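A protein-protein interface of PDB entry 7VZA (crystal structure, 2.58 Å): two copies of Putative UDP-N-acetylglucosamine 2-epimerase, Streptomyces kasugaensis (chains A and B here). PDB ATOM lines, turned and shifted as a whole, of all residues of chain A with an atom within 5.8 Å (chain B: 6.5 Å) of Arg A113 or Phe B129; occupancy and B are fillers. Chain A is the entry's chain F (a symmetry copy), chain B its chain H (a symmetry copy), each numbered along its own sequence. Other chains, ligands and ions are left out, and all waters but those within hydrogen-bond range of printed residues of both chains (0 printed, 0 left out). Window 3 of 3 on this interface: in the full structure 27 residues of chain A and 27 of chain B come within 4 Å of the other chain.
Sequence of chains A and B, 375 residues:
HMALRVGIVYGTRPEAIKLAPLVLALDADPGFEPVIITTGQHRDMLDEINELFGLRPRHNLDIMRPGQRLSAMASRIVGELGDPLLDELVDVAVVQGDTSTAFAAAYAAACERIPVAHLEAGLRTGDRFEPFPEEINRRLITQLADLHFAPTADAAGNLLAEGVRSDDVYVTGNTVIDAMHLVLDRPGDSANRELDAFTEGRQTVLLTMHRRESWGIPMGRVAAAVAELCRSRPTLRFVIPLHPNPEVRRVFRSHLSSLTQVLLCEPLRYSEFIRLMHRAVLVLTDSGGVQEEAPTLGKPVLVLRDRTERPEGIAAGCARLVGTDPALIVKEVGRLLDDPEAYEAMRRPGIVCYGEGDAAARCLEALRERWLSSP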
ATOM      1  N   ASP A  91       6.329  21.339  -5.939  1.00  0.00           N
ATOM      2  CA  ASP A  91       7.480  20.925  -6.778  1.00  0.00           C
ATOM      3  C   ASP A  91       6.966  20.183  -8.013  1.00  0.00           C
ATOM      4  O   ASP A  91       7.621  20.273  -9.067  1.00  0.00           O
ATOM      5  CB  ASP A  91       8.445  20.027  -5.994  1.00  0.00           C
ATOM      6  CG  ASP A  91       9.092  20.697  -4.788  1.00  0.00           C
ATOM      7  OD1 ASP A  91       9.593  21.847  -4.937  1.00  0.00           O
ATOM      8  OD2 ASP A  91       9.091  20.065  -3.717  1.00  0.00           O
ATOM      9  N   ALA A 108      -1.729  25.349 -16.250  1.00  0.00           N
ATOM     10  CA  ALA A 108      -1.339  26.335 -15.214  1.00  0.00           C
ATOM     11  C   ALA A 108      -0.005  25.919 -14.601  1.00  0.00           C
ATOM     12  O   ALA A 108       0.889  26.769 -14.483  1.00  0.00           O
ATOM     13  CB  ALA A 108      -2.401  26.448 -14.149  1.00  0.00           C
ATOM     14  N   ALA A 109       0.131  24.651 -14.216  1.00  0.00           N
ATOM     15  CA  ALA A 109       1.376  24.115 -13.638  1.00  0.00           C
ATOM     16  C   ALA A 109       2.518  24.357 -14.628  1.00  0.00           C
ATOM     17  O   ALA A 109       3.578  24.863 -14.210  1.00  0.00           O
ATOM     18  CB  ALA A 109       1.212  22.663 -13.303  1.00  0.00           C
ATOM     19  N   ALA A 110       2.304  24.038 -15.906  1.00  0.00           N
ATOM     20  CA  ALA A 110       3.343  24.121 -16.957  1.00  0.00           C
ATOM     21  C   ALA A 110       3.792  25.577 -17.129  1.00  0.00           C
ATOM     22  O   ALA A 110       5.004  25.786 -17.317  1.00  0.00           O
ATOM     23  CB  ALA A 110       2.832  23.541 -18.251  1.00  0.00           C
ATOM     24  N   CYS A 111       2.865  26.539 -17.058  1.00  0.00           N
ATOM     25  CA  CYS A 111       3.168  27.998 -17.127  1.00  0.00           C
ATOM     26  C   CYS A 111       4.169  28.398 -16.034  1.00  0.00           C
ATOM     27  O   CYS A 111       5.009  29.256 -16.313  1.00  0.00           O
ATOM     28  CB  CYS A 111       1.913  28.849 -17.008  1.00  0.00           C
ATOM     29  SG  CYS A 111       0.852  28.719 -18.462  1.00  0.00           S
ATOM     30  N   GLU A 112       4.089  27.788 -14.842  1.00  0.00           N
ATOM     31  CA  GLU A 112       4.998  28.065 -13.697  1.00  0.00           C
ATOM     32  C   GLU A 112       6.189  27.105 -13.710  1.00  0.00           C
ATOM     33  O   GLU A 112       6.887  27.044 -12.691  1.00  0.00           O
ATOM     34  CB  GLU A 112       4.247  27.952 -12.366  1.00  0.00           C
ATOM     35  CG  GLU A 112       3.014  28.842 -12.265  1.00  0.00           C
ATOM     36  CD  GLU A 112       3.207  30.297 -12.672  1.00  0.00           C
ATOM     37  OE1 GLU A 112       4.324  30.832 -12.462  1.00  0.00           O
ATOM     38  OE2 GLU A 112       2.244  30.890 -13.217  1.00  0.00           O
ATOM     39  N   ARG A 113       6.413  26.378 -14.807  1.00  0.00           N
ATOM     40  CA  ARG A 113       7.520  25.387 -14.958  1.00  0.00           C
ATOM     41  C   ARG A 113       7.469  24.349 -13.826  1.00  0.00           C
ATOM     42  O   ARG A 113       8.537  23.823 -13.459  1.00  0.00           O
ATOM     43  CB  ARG A 113       8.890  26.079 -14.983  1.00  0.00           C
ATOM     44  CG  ARG A 113       9.045  27.178 -16.028  1.00  0.00           C
ATOM     45  CD  ARG A 113       8.592  26.779 -17.427  1.00  0.00           C
ATOM     46  NE  ARG A 113       8.974  25.418 -17.843  1.00  0.00           N
ATOM     47  CZ  ARG A 113      10.102  25.078 -18.476  1.00  0.00           C
ATOM     48  NH1 ARG A 113      11.017  25.992 -18.767  1.00  0.00           N
ATOM     49  NH2 ARG A 113      10.303  23.815 -18.821  1.00  0.00           N
ATOM     50  N   ILE A 114       6.274  24.053 -13.309  1.00  0.00           N
ATOM     51  CA  ILE A 114       6.011  22.939 -12.351  1.00  0.00           C
ATOM     52  C   ILE A 114       5.764  21.670 -13.159  1.00  0.00           C
ATOM     53  O   ILE A 114       4.783  21.573 -13.890  1.00  0.00           O
ATOM     54  CB  ILE A 114       4.811  23.266 -11.437  1.00  0.00           C
ATOM     55  CG1 ILE A 114       5.106  24.484 -10.557  1.00  0.00           C
ATOM     56  CG2 ILE A 114       4.402  22.044 -10.609  1.00  0.00           C
ATOM     57  CD1 ILE A 114       3.885  25.086  -9.919  1.00  0.00           C
ATOM     58  N   PRO A 115       6.646  20.651 -13.064  1.00  0.00           N
ATOM     59  CA  PRO A 115       6.421  19.383 -13.752  1.00  0.00           C
ATOM     60  C   PRO A 115       5.076  18.762 -13.353  1.00  0.00           C
ATOM     61  O   PRO A 115       4.661  18.941 -12.225  1.00  0.00           O
ATOM     62  CB  PRO A 115       7.586  18.505 -13.287  1.00  0.00           C
ATOM     63  CG  PRO A 115       8.660  19.484 -12.870  1.00  0.00           C
ATOM     64  CD  PRO A 115       7.910  20.669 -12.315  1.00  0.00           C
ATOM     65  N   GLN A 143       0.432  15.575 -23.561  1.00  0.00           N
ATOM     66  CA  GLN A 143       1.589  16.376 -24.054  1.00  0.00           C
ATOM     67  C   GLN A 143       2.170  17.233 -22.920  1.00  0.00           C
ATOM     68  O   GLN A 143       3.368  17.517 -22.980  1.00  0.00           O
ATOM     69  CB  GLN A 143       1.199  17.252 -25.250  1.00  0.00           C
ATOM     70  CG  GLN A 143       0.720  16.469 -26.463  1.00  0.00           C
ATOM     71  CD  GLN A 143       1.714  15.445 -26.966  1.00  0.00           C
ATOM     72  OE1 GLN A 143       2.904  15.706 -27.104  1.00  0.00           O
ATOM     73  NE2 GLN A 143       1.212  14.261 -27.272  1.00  0.00           N
ATOM     74  N   LEU A 144       1.363  17.633 -21.932  1.00  0.00           N
ATOM     75  CA  LEU A 144       1.813  18.527 -20.826  1.00  0.00           C
ATOM     76  C   LEU A 144       2.568  17.705 -19.773  1.00  0.00           C
ATOM     77  O   LEU A 144       3.581  18.212 -19.252  1.00  0.00           O
ATOM     78  CB  LEU A 144       0.610  19.240 -20.203  1.00  0.00           C
ATOM     79  CG  LEU A 144       0.038  20.389 -21.027  1.00  0.00           C
ATOM     80  CD1 LEU A 144      -1.398  20.695 -20.636  1.00  0.00           C
ATOM     81  CD2 LEU A 144       0.905  21.635 -20.926  1.00  0.00           C
ATOM     82  N   ASP A 146       4.974  15.210 -17.721  1.00  0.00           N
ATOM     83  CA  ASP A 146       6.347  14.634 -17.802  1.00  0.00           C
ATOM     84  C   ASP A 146       6.278  13.135 -17.495  1.00  0.00           C
ATOM     85  O   ASP A 146       7.127  12.388 -18.013  1.00  0.00           O
ATOM     86  CB  ASP A 146       7.329  15.304 -16.843  1.00  0.00           C
ATOM     87  CG  ASP A 146       7.717  16.734 -17.179  1.00  0.00           C
ATOM     88  OD1 ASP A 146       7.195  17.281 -18.180  1.00  0.00           O
ATOM     89  OD2 ASP A 146       8.517  17.304 -16.407  1.00  0.00           O
ATOM     90  N   ASP B 127      13.963  18.217 -28.555  1.00  0.00           N
ATOM     91  CA  ASP B 127      14.377  18.462 -27.143  1.00  0.00           C
ATOM     92  C   ASP B 127      13.176  19.056 -26.392  1.00  0.00           C
ATOM     93  O   ASP B 127      12.664  20.113 -26.827  1.00  0.00           O
ATOM     94  CB  ASP B 127      15.634  19.340 -27.100  1.00  0.00           C
ATOM     95  CG  ASP B 127      16.731  18.894 -28.068  1.00  0.00           C
ATOM     96  OD1 ASP B 127      16.774  17.686 -28.380  1.00  0.00           O
ATOM     97  OD2 ASP B 127      17.525  19.754 -28.532  1.00  0.00           O
ATOM     98  N   ARG B 128      12.735  18.389 -25.318  1.00  0.00           N
ATOM     99  CA  ARG B 128      11.455  18.662 -24.603  1.00  0.00           C
ATOM    100  C   ARG B 128      11.515  20.015 -23.876  1.00  0.00           C
ATOM    101  O   ARG B 128      12.518  20.263 -23.181  1.00  0.00           O
ATOM    102  CB  ARG B 128      11.163  17.513 -23.633  1.00  0.00           C
ATOM    103  CG  ARG B 128       9.863  17.666 -22.859  1.00  0.00           C
ATOM    104  CD  ARG B 128       9.532  16.462 -21.991  1.00  0.00           C
ATOM    105  NE  ARG B 128       8.281  16.637 -21.263  1.00  0.00           N
ATOM    106  CZ  ARG B 128       7.059  16.549 -21.797  1.00  0.00           C
ATOM    107  NH1 ARG B 128       6.892  16.284 -23.086  1.00  0.00           N
ATOM    108  NH2 ARG B 128       5.998  16.750 -21.034  1.00  0.00           N
ATOM    109  N   PHE B 129      10.464  20.841 -24.020  1.00  0.00           N
ATOM    110  CA  PHE B 129      10.287  22.185 -23.391  1.00  0.00           C
ATOM    111  C   PHE B 129      11.450  23.116 -23.771  1.00  0.00           C
ATOM    112  O   PHE B 129      11.722  24.079 -23.036  1.00  0.00           O
ATOM    113  CB  PHE B 129      10.122  22.080 -21.865  1.00  0.00           C
ATOM    114  CG  PHE B 129       8.831  21.466 -21.368  1.00  0.00           C
ATOM    115  CD1 PHE B 129       7.606  21.778 -21.950  1.00  0.00           C
ATOM    116  CD2 PHE B 129       8.830  20.601 -20.280  1.00  0.00           C
ATOM    117  CE1 PHE B 129       6.429  21.206 -21.488  1.00  0.00           C
ATOM    118  CE2 PHE B 129       7.650  20.038 -19.819  1.00  0.00           C
ATOM    119  CZ  PHE B 129       6.450  20.344 -20.420  1.00  0.00           C
ATOM    120  N   GLU B 130      12.094  22.851 -24.909  1.00  0.00           N
ATOM    121  CA  GLU B 130      13.282  23.581 -25.419  1.00  0.00           C
ATOM    122  C   GLU B 130      13.053  23.945 -26.885  1.00  0.00           C
ATOM    123  O   GLU B 130      13.183  23.088 -27.759  1.00  0.00           O
ATOM    124  CB  GLU B 130      14.539  22.715 -25.276  1.00  0.00           C
ATOM    125  CG  GLU B 130      14.922  22.428 -23.831  1.00  0.00           C
ATOM    126  CD  GLU B 130      16.421  22.333 -23.567  1.00  0.00           C
ATOM    127  OE1 GLU B 130      17.023  21.276 -23.845  1.00  0.00           O
ATOM    128  OE2 GLU B 130      16.979  23.332 -23.115  1.00  0.00           O
ATOM    129  N   PRO B 131      12.685  25.205 -27.220  1.00  0.00           N
ATOM    130  CA  PRO B 131      12.457  26.268 -26.239  1.00  0.00           C
ATOM    131  C   PRO B 131      11.071  26.202 -25.576  1.00  0.00           C
ATOM    132  O   PRO B 131      10.212  25.481 -26.068  1.00  0.00           O
ATOM    133  CB  PRO B 131      12.600  27.547 -27.086  1.00  0.00           C
ATOM    134  CG  PRO B 131      12.165  27.139 -28.485  1.00  0.00           C
ATOM    135  CD  PRO B 131      12.485  25.666 -28.603  1.00  0.00           C
ATOM    136  N   PHE B 132      10.882  26.943 -24.477  1.00  0.00           N
ATOM    137  CA  PHE B 132       9.586  27.051 -23.756  1.00  0.00           C
ATOM    138  C   PHE B 132       9.048  28.461 -23.937  1.00  0.00           C
ATOM    139  O   PHE B 132       9.785  29.420 -23.751  1.00  0.00           O
ATOM    140  CB  PHE B 132       9.716  26.728 -22.265  1.00  0.00           C
ATOM    141  CG  PHE B 132       8.400  26.767 -21.526  1.00  0.00           C
ATOM    142  CD1 PHE B 132       7.902  27.962 -21.023  1.00  0.00           C
ATOM    143  CD2 PHE B 132       7.635  25.617 -21.366  1.00  0.00           C
ATOM    144  CE1 PHE B 132       6.682  28.000 -20.363  1.00  0.00           C
ATOM    145  CE2 PHE B 132       6.416  25.659 -20.703  1.00  0.00           C
ATOM    146  CZ  PHE B 132       5.936  26.850 -20.206  1.00  0.00           C
ATOM    147  N   PRO B 133       7.752  28.643 -24.274  1.00  0.00           N
ATOM    148  CA  PRO B 133       6.801  27.536 -24.413  1.00  0.00           C
ATOM    149  C   PRO B 133       6.540  27.009 -25.837  1.00  0.00           C
ATOM    150  O   PRO B 133       5.585  26.275 -26.019  1.00  0.00           O
ATOM    151  CB  PRO B 133       5.537  28.219 -23.874  1.00  0.00           C
ATOM    152  CG  PRO B 133       5.636  29.635 -24.423  1.00  0.00           C
ATOM    153  CD  PRO B 133       7.116  29.948 -24.519  1.00  0.00           C
ATOM    154  N   GLU B 135       7.748  24.793 -27.986  1.00  0.00           N
ATOM    155  CA  GLU B 135       7.773  23.347 -28.310  1.00  0.00           C
ATOM    156  C   GLU B 135       6.499  22.702 -27.763  1.00  0.00           C
ATOM    157  O   GLU B 135       5.901  21.899 -28.492  1.00  0.00           O
ATOM    158  CB  GLU B 135       9.055  22.703 -27.784  1.00  0.00           C
ATOM    159  CG  GLU B 135       9.444  21.442 -28.533  1.00  0.00           C
ATOM    160  CD  GLU B 135       8.956  20.125 -27.944  1.00  0.00           C
ATOM    161  OE1 GLU B 135       8.633  20.084 -26.712  1.00  0.00           O
ATOM    162  OE2 GLU B 135       8.895  19.137 -28.735  1.00  0.00           O
ATOM    163  N   ILE B 136       6.085  23.046 -26.545  1.00  0.00           N
ATOM    164  CA  ILE B 136       4.841  22.474 -25.937  1.00  0.00           C
ATOM    165  C   ILE B 136       3.607  23.033 -26.673  1.00  0.00           C
ATOM    166  O   ILE B 136       2.646  22.291 -26.859  1.00  0.00           O
ATOM    167  CB  ILE B 136       4.785  22.690 -24.409  1.00  0.00           C
ATOM    168  CG1 ILE B 136       3.504  22.126 -23.789  1.00  0.00           C
ATOM    169  CG2 ILE B 136       4.946  24.151 -24.045  1.00  0.00           C
ATOM    170  CD1 ILE B 136       3.301  20.651 -24.015  1.00  0.00           C
ATOM    171  N   ARG B 139       2.889  20.989 -29.789  1.00  0.00           N
ATOM    172  CA  ARG B 139       2.350  19.649 -29.448  1.00  0.00           C
ATOM    173  C   ARG B 139       0.891  19.767 -28.980  1.00  0.00           C
ATOM    174  O   ARG B 139       0.108  18.835 -29.259  1.00  0.00           O
ATOM    175  CB  ARG B 139       3.284  18.955 -28.452  1.00  0.00           C
ATOM    176  CG  ARG B 139       4.612  18.562 -29.096  1.00  0.00           C
ATOM    177  CD  ARG B 139       5.386  17.501 -28.345  1.00  0.00           C
ATOM    178  NE  ARG B 139       6.097  18.112 -27.241  1.00  0.00           N
ATOM    179  CZ  ARG B 139       5.731  18.067 -25.975  1.00  0.00           C
ATOM    180  NH1 ARG B 139       4.644  17.409 -25.606  1.00  0.00           N
ATOM    181  NH2 ARG B 139       6.470  18.685 -25.071  1.00  0.00           N
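O of Gln A143 sits at hydrogen-bond distance from NH2 of Arg B128 (3.4 Å).
The side-chain amide oxygen (OE1) of Gln A143 sits at hydrogen-bond distance from the guanidinium group (NH1) of Arg B139 (2.9 Å).
O of Leu A144 is in hydrogen-bond range of NH2 of Arg B128 (3.3 Å).
OD1 of Asp A146 lies within salt-bridge range of NH2 of Arg B128, 3.1 Å away.
The side-chain carboxylate (OE1) of Glu B135 is in hydrogen-bond range of the backbone NH (N) of Phe B129, at 3.3 Å.
The guanidinium group (NH2) of Arg B139 lies within salt-bridge range of the side-chain carboxylate (OE1) of Glu B135.
Among the printed residues, merely in contact across the chains: Ala A110 with Phe B132 (3.2 Å), Asp A146 with Phe B129 (3.2 Å), Gln A143 with Ile B136 (3.3 Å), Arg A113 with Phe B129 (3.5 Å), Arg A113 with Phe B132 (3.7 Å), Leu A144 with Phe B129 (3.8 Å) and Leu A144 with Ile B136 (3.9 Å).
Asp A91 touches none of the printed residues of chain B.
Arg A113 touches just these residues of chain B: Phe B129 and Phe B132.
Of the printed residues of chain B, Leu A144 touches Arg B128, Phe B129 and Ile B136.
Of the printed residues of chain A, Arg B128 touches Gln A143, Leu A144 and Asp A146.
Of the printed residues of chain A, Phe B129 touches Arg A113 (3.5 Å), Leu A144 (3.8 Å) and Asp A146 (3.2 Å).
Of the printed residues of chain A, Ile B136 touches Gln A143 (3.3 Å) and Leu A144 (3.9 Å).
The nearest residue of chain B that does not touch Arg A113 is Arg B128 (6.0 Å).
Of the 12 printed residues of chain A, 5 touch a printed residue of chain B.
Of the 10 printed residues of chain B, 5 touch a printed residue of chain A.
Printed residues of chain B that touch a printed residue of chain A: Arg B128, Phe B129, Phe B132, Ile B136 and Arg B139.
Hydrophobic or aromatic side chains of chain B within 4 Å of the printed part of chain A: Phe B129, Phe B132 and Ile B136.
Among the printed residues, 11 pairs touch across the chains.
No position is printed for both chains.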
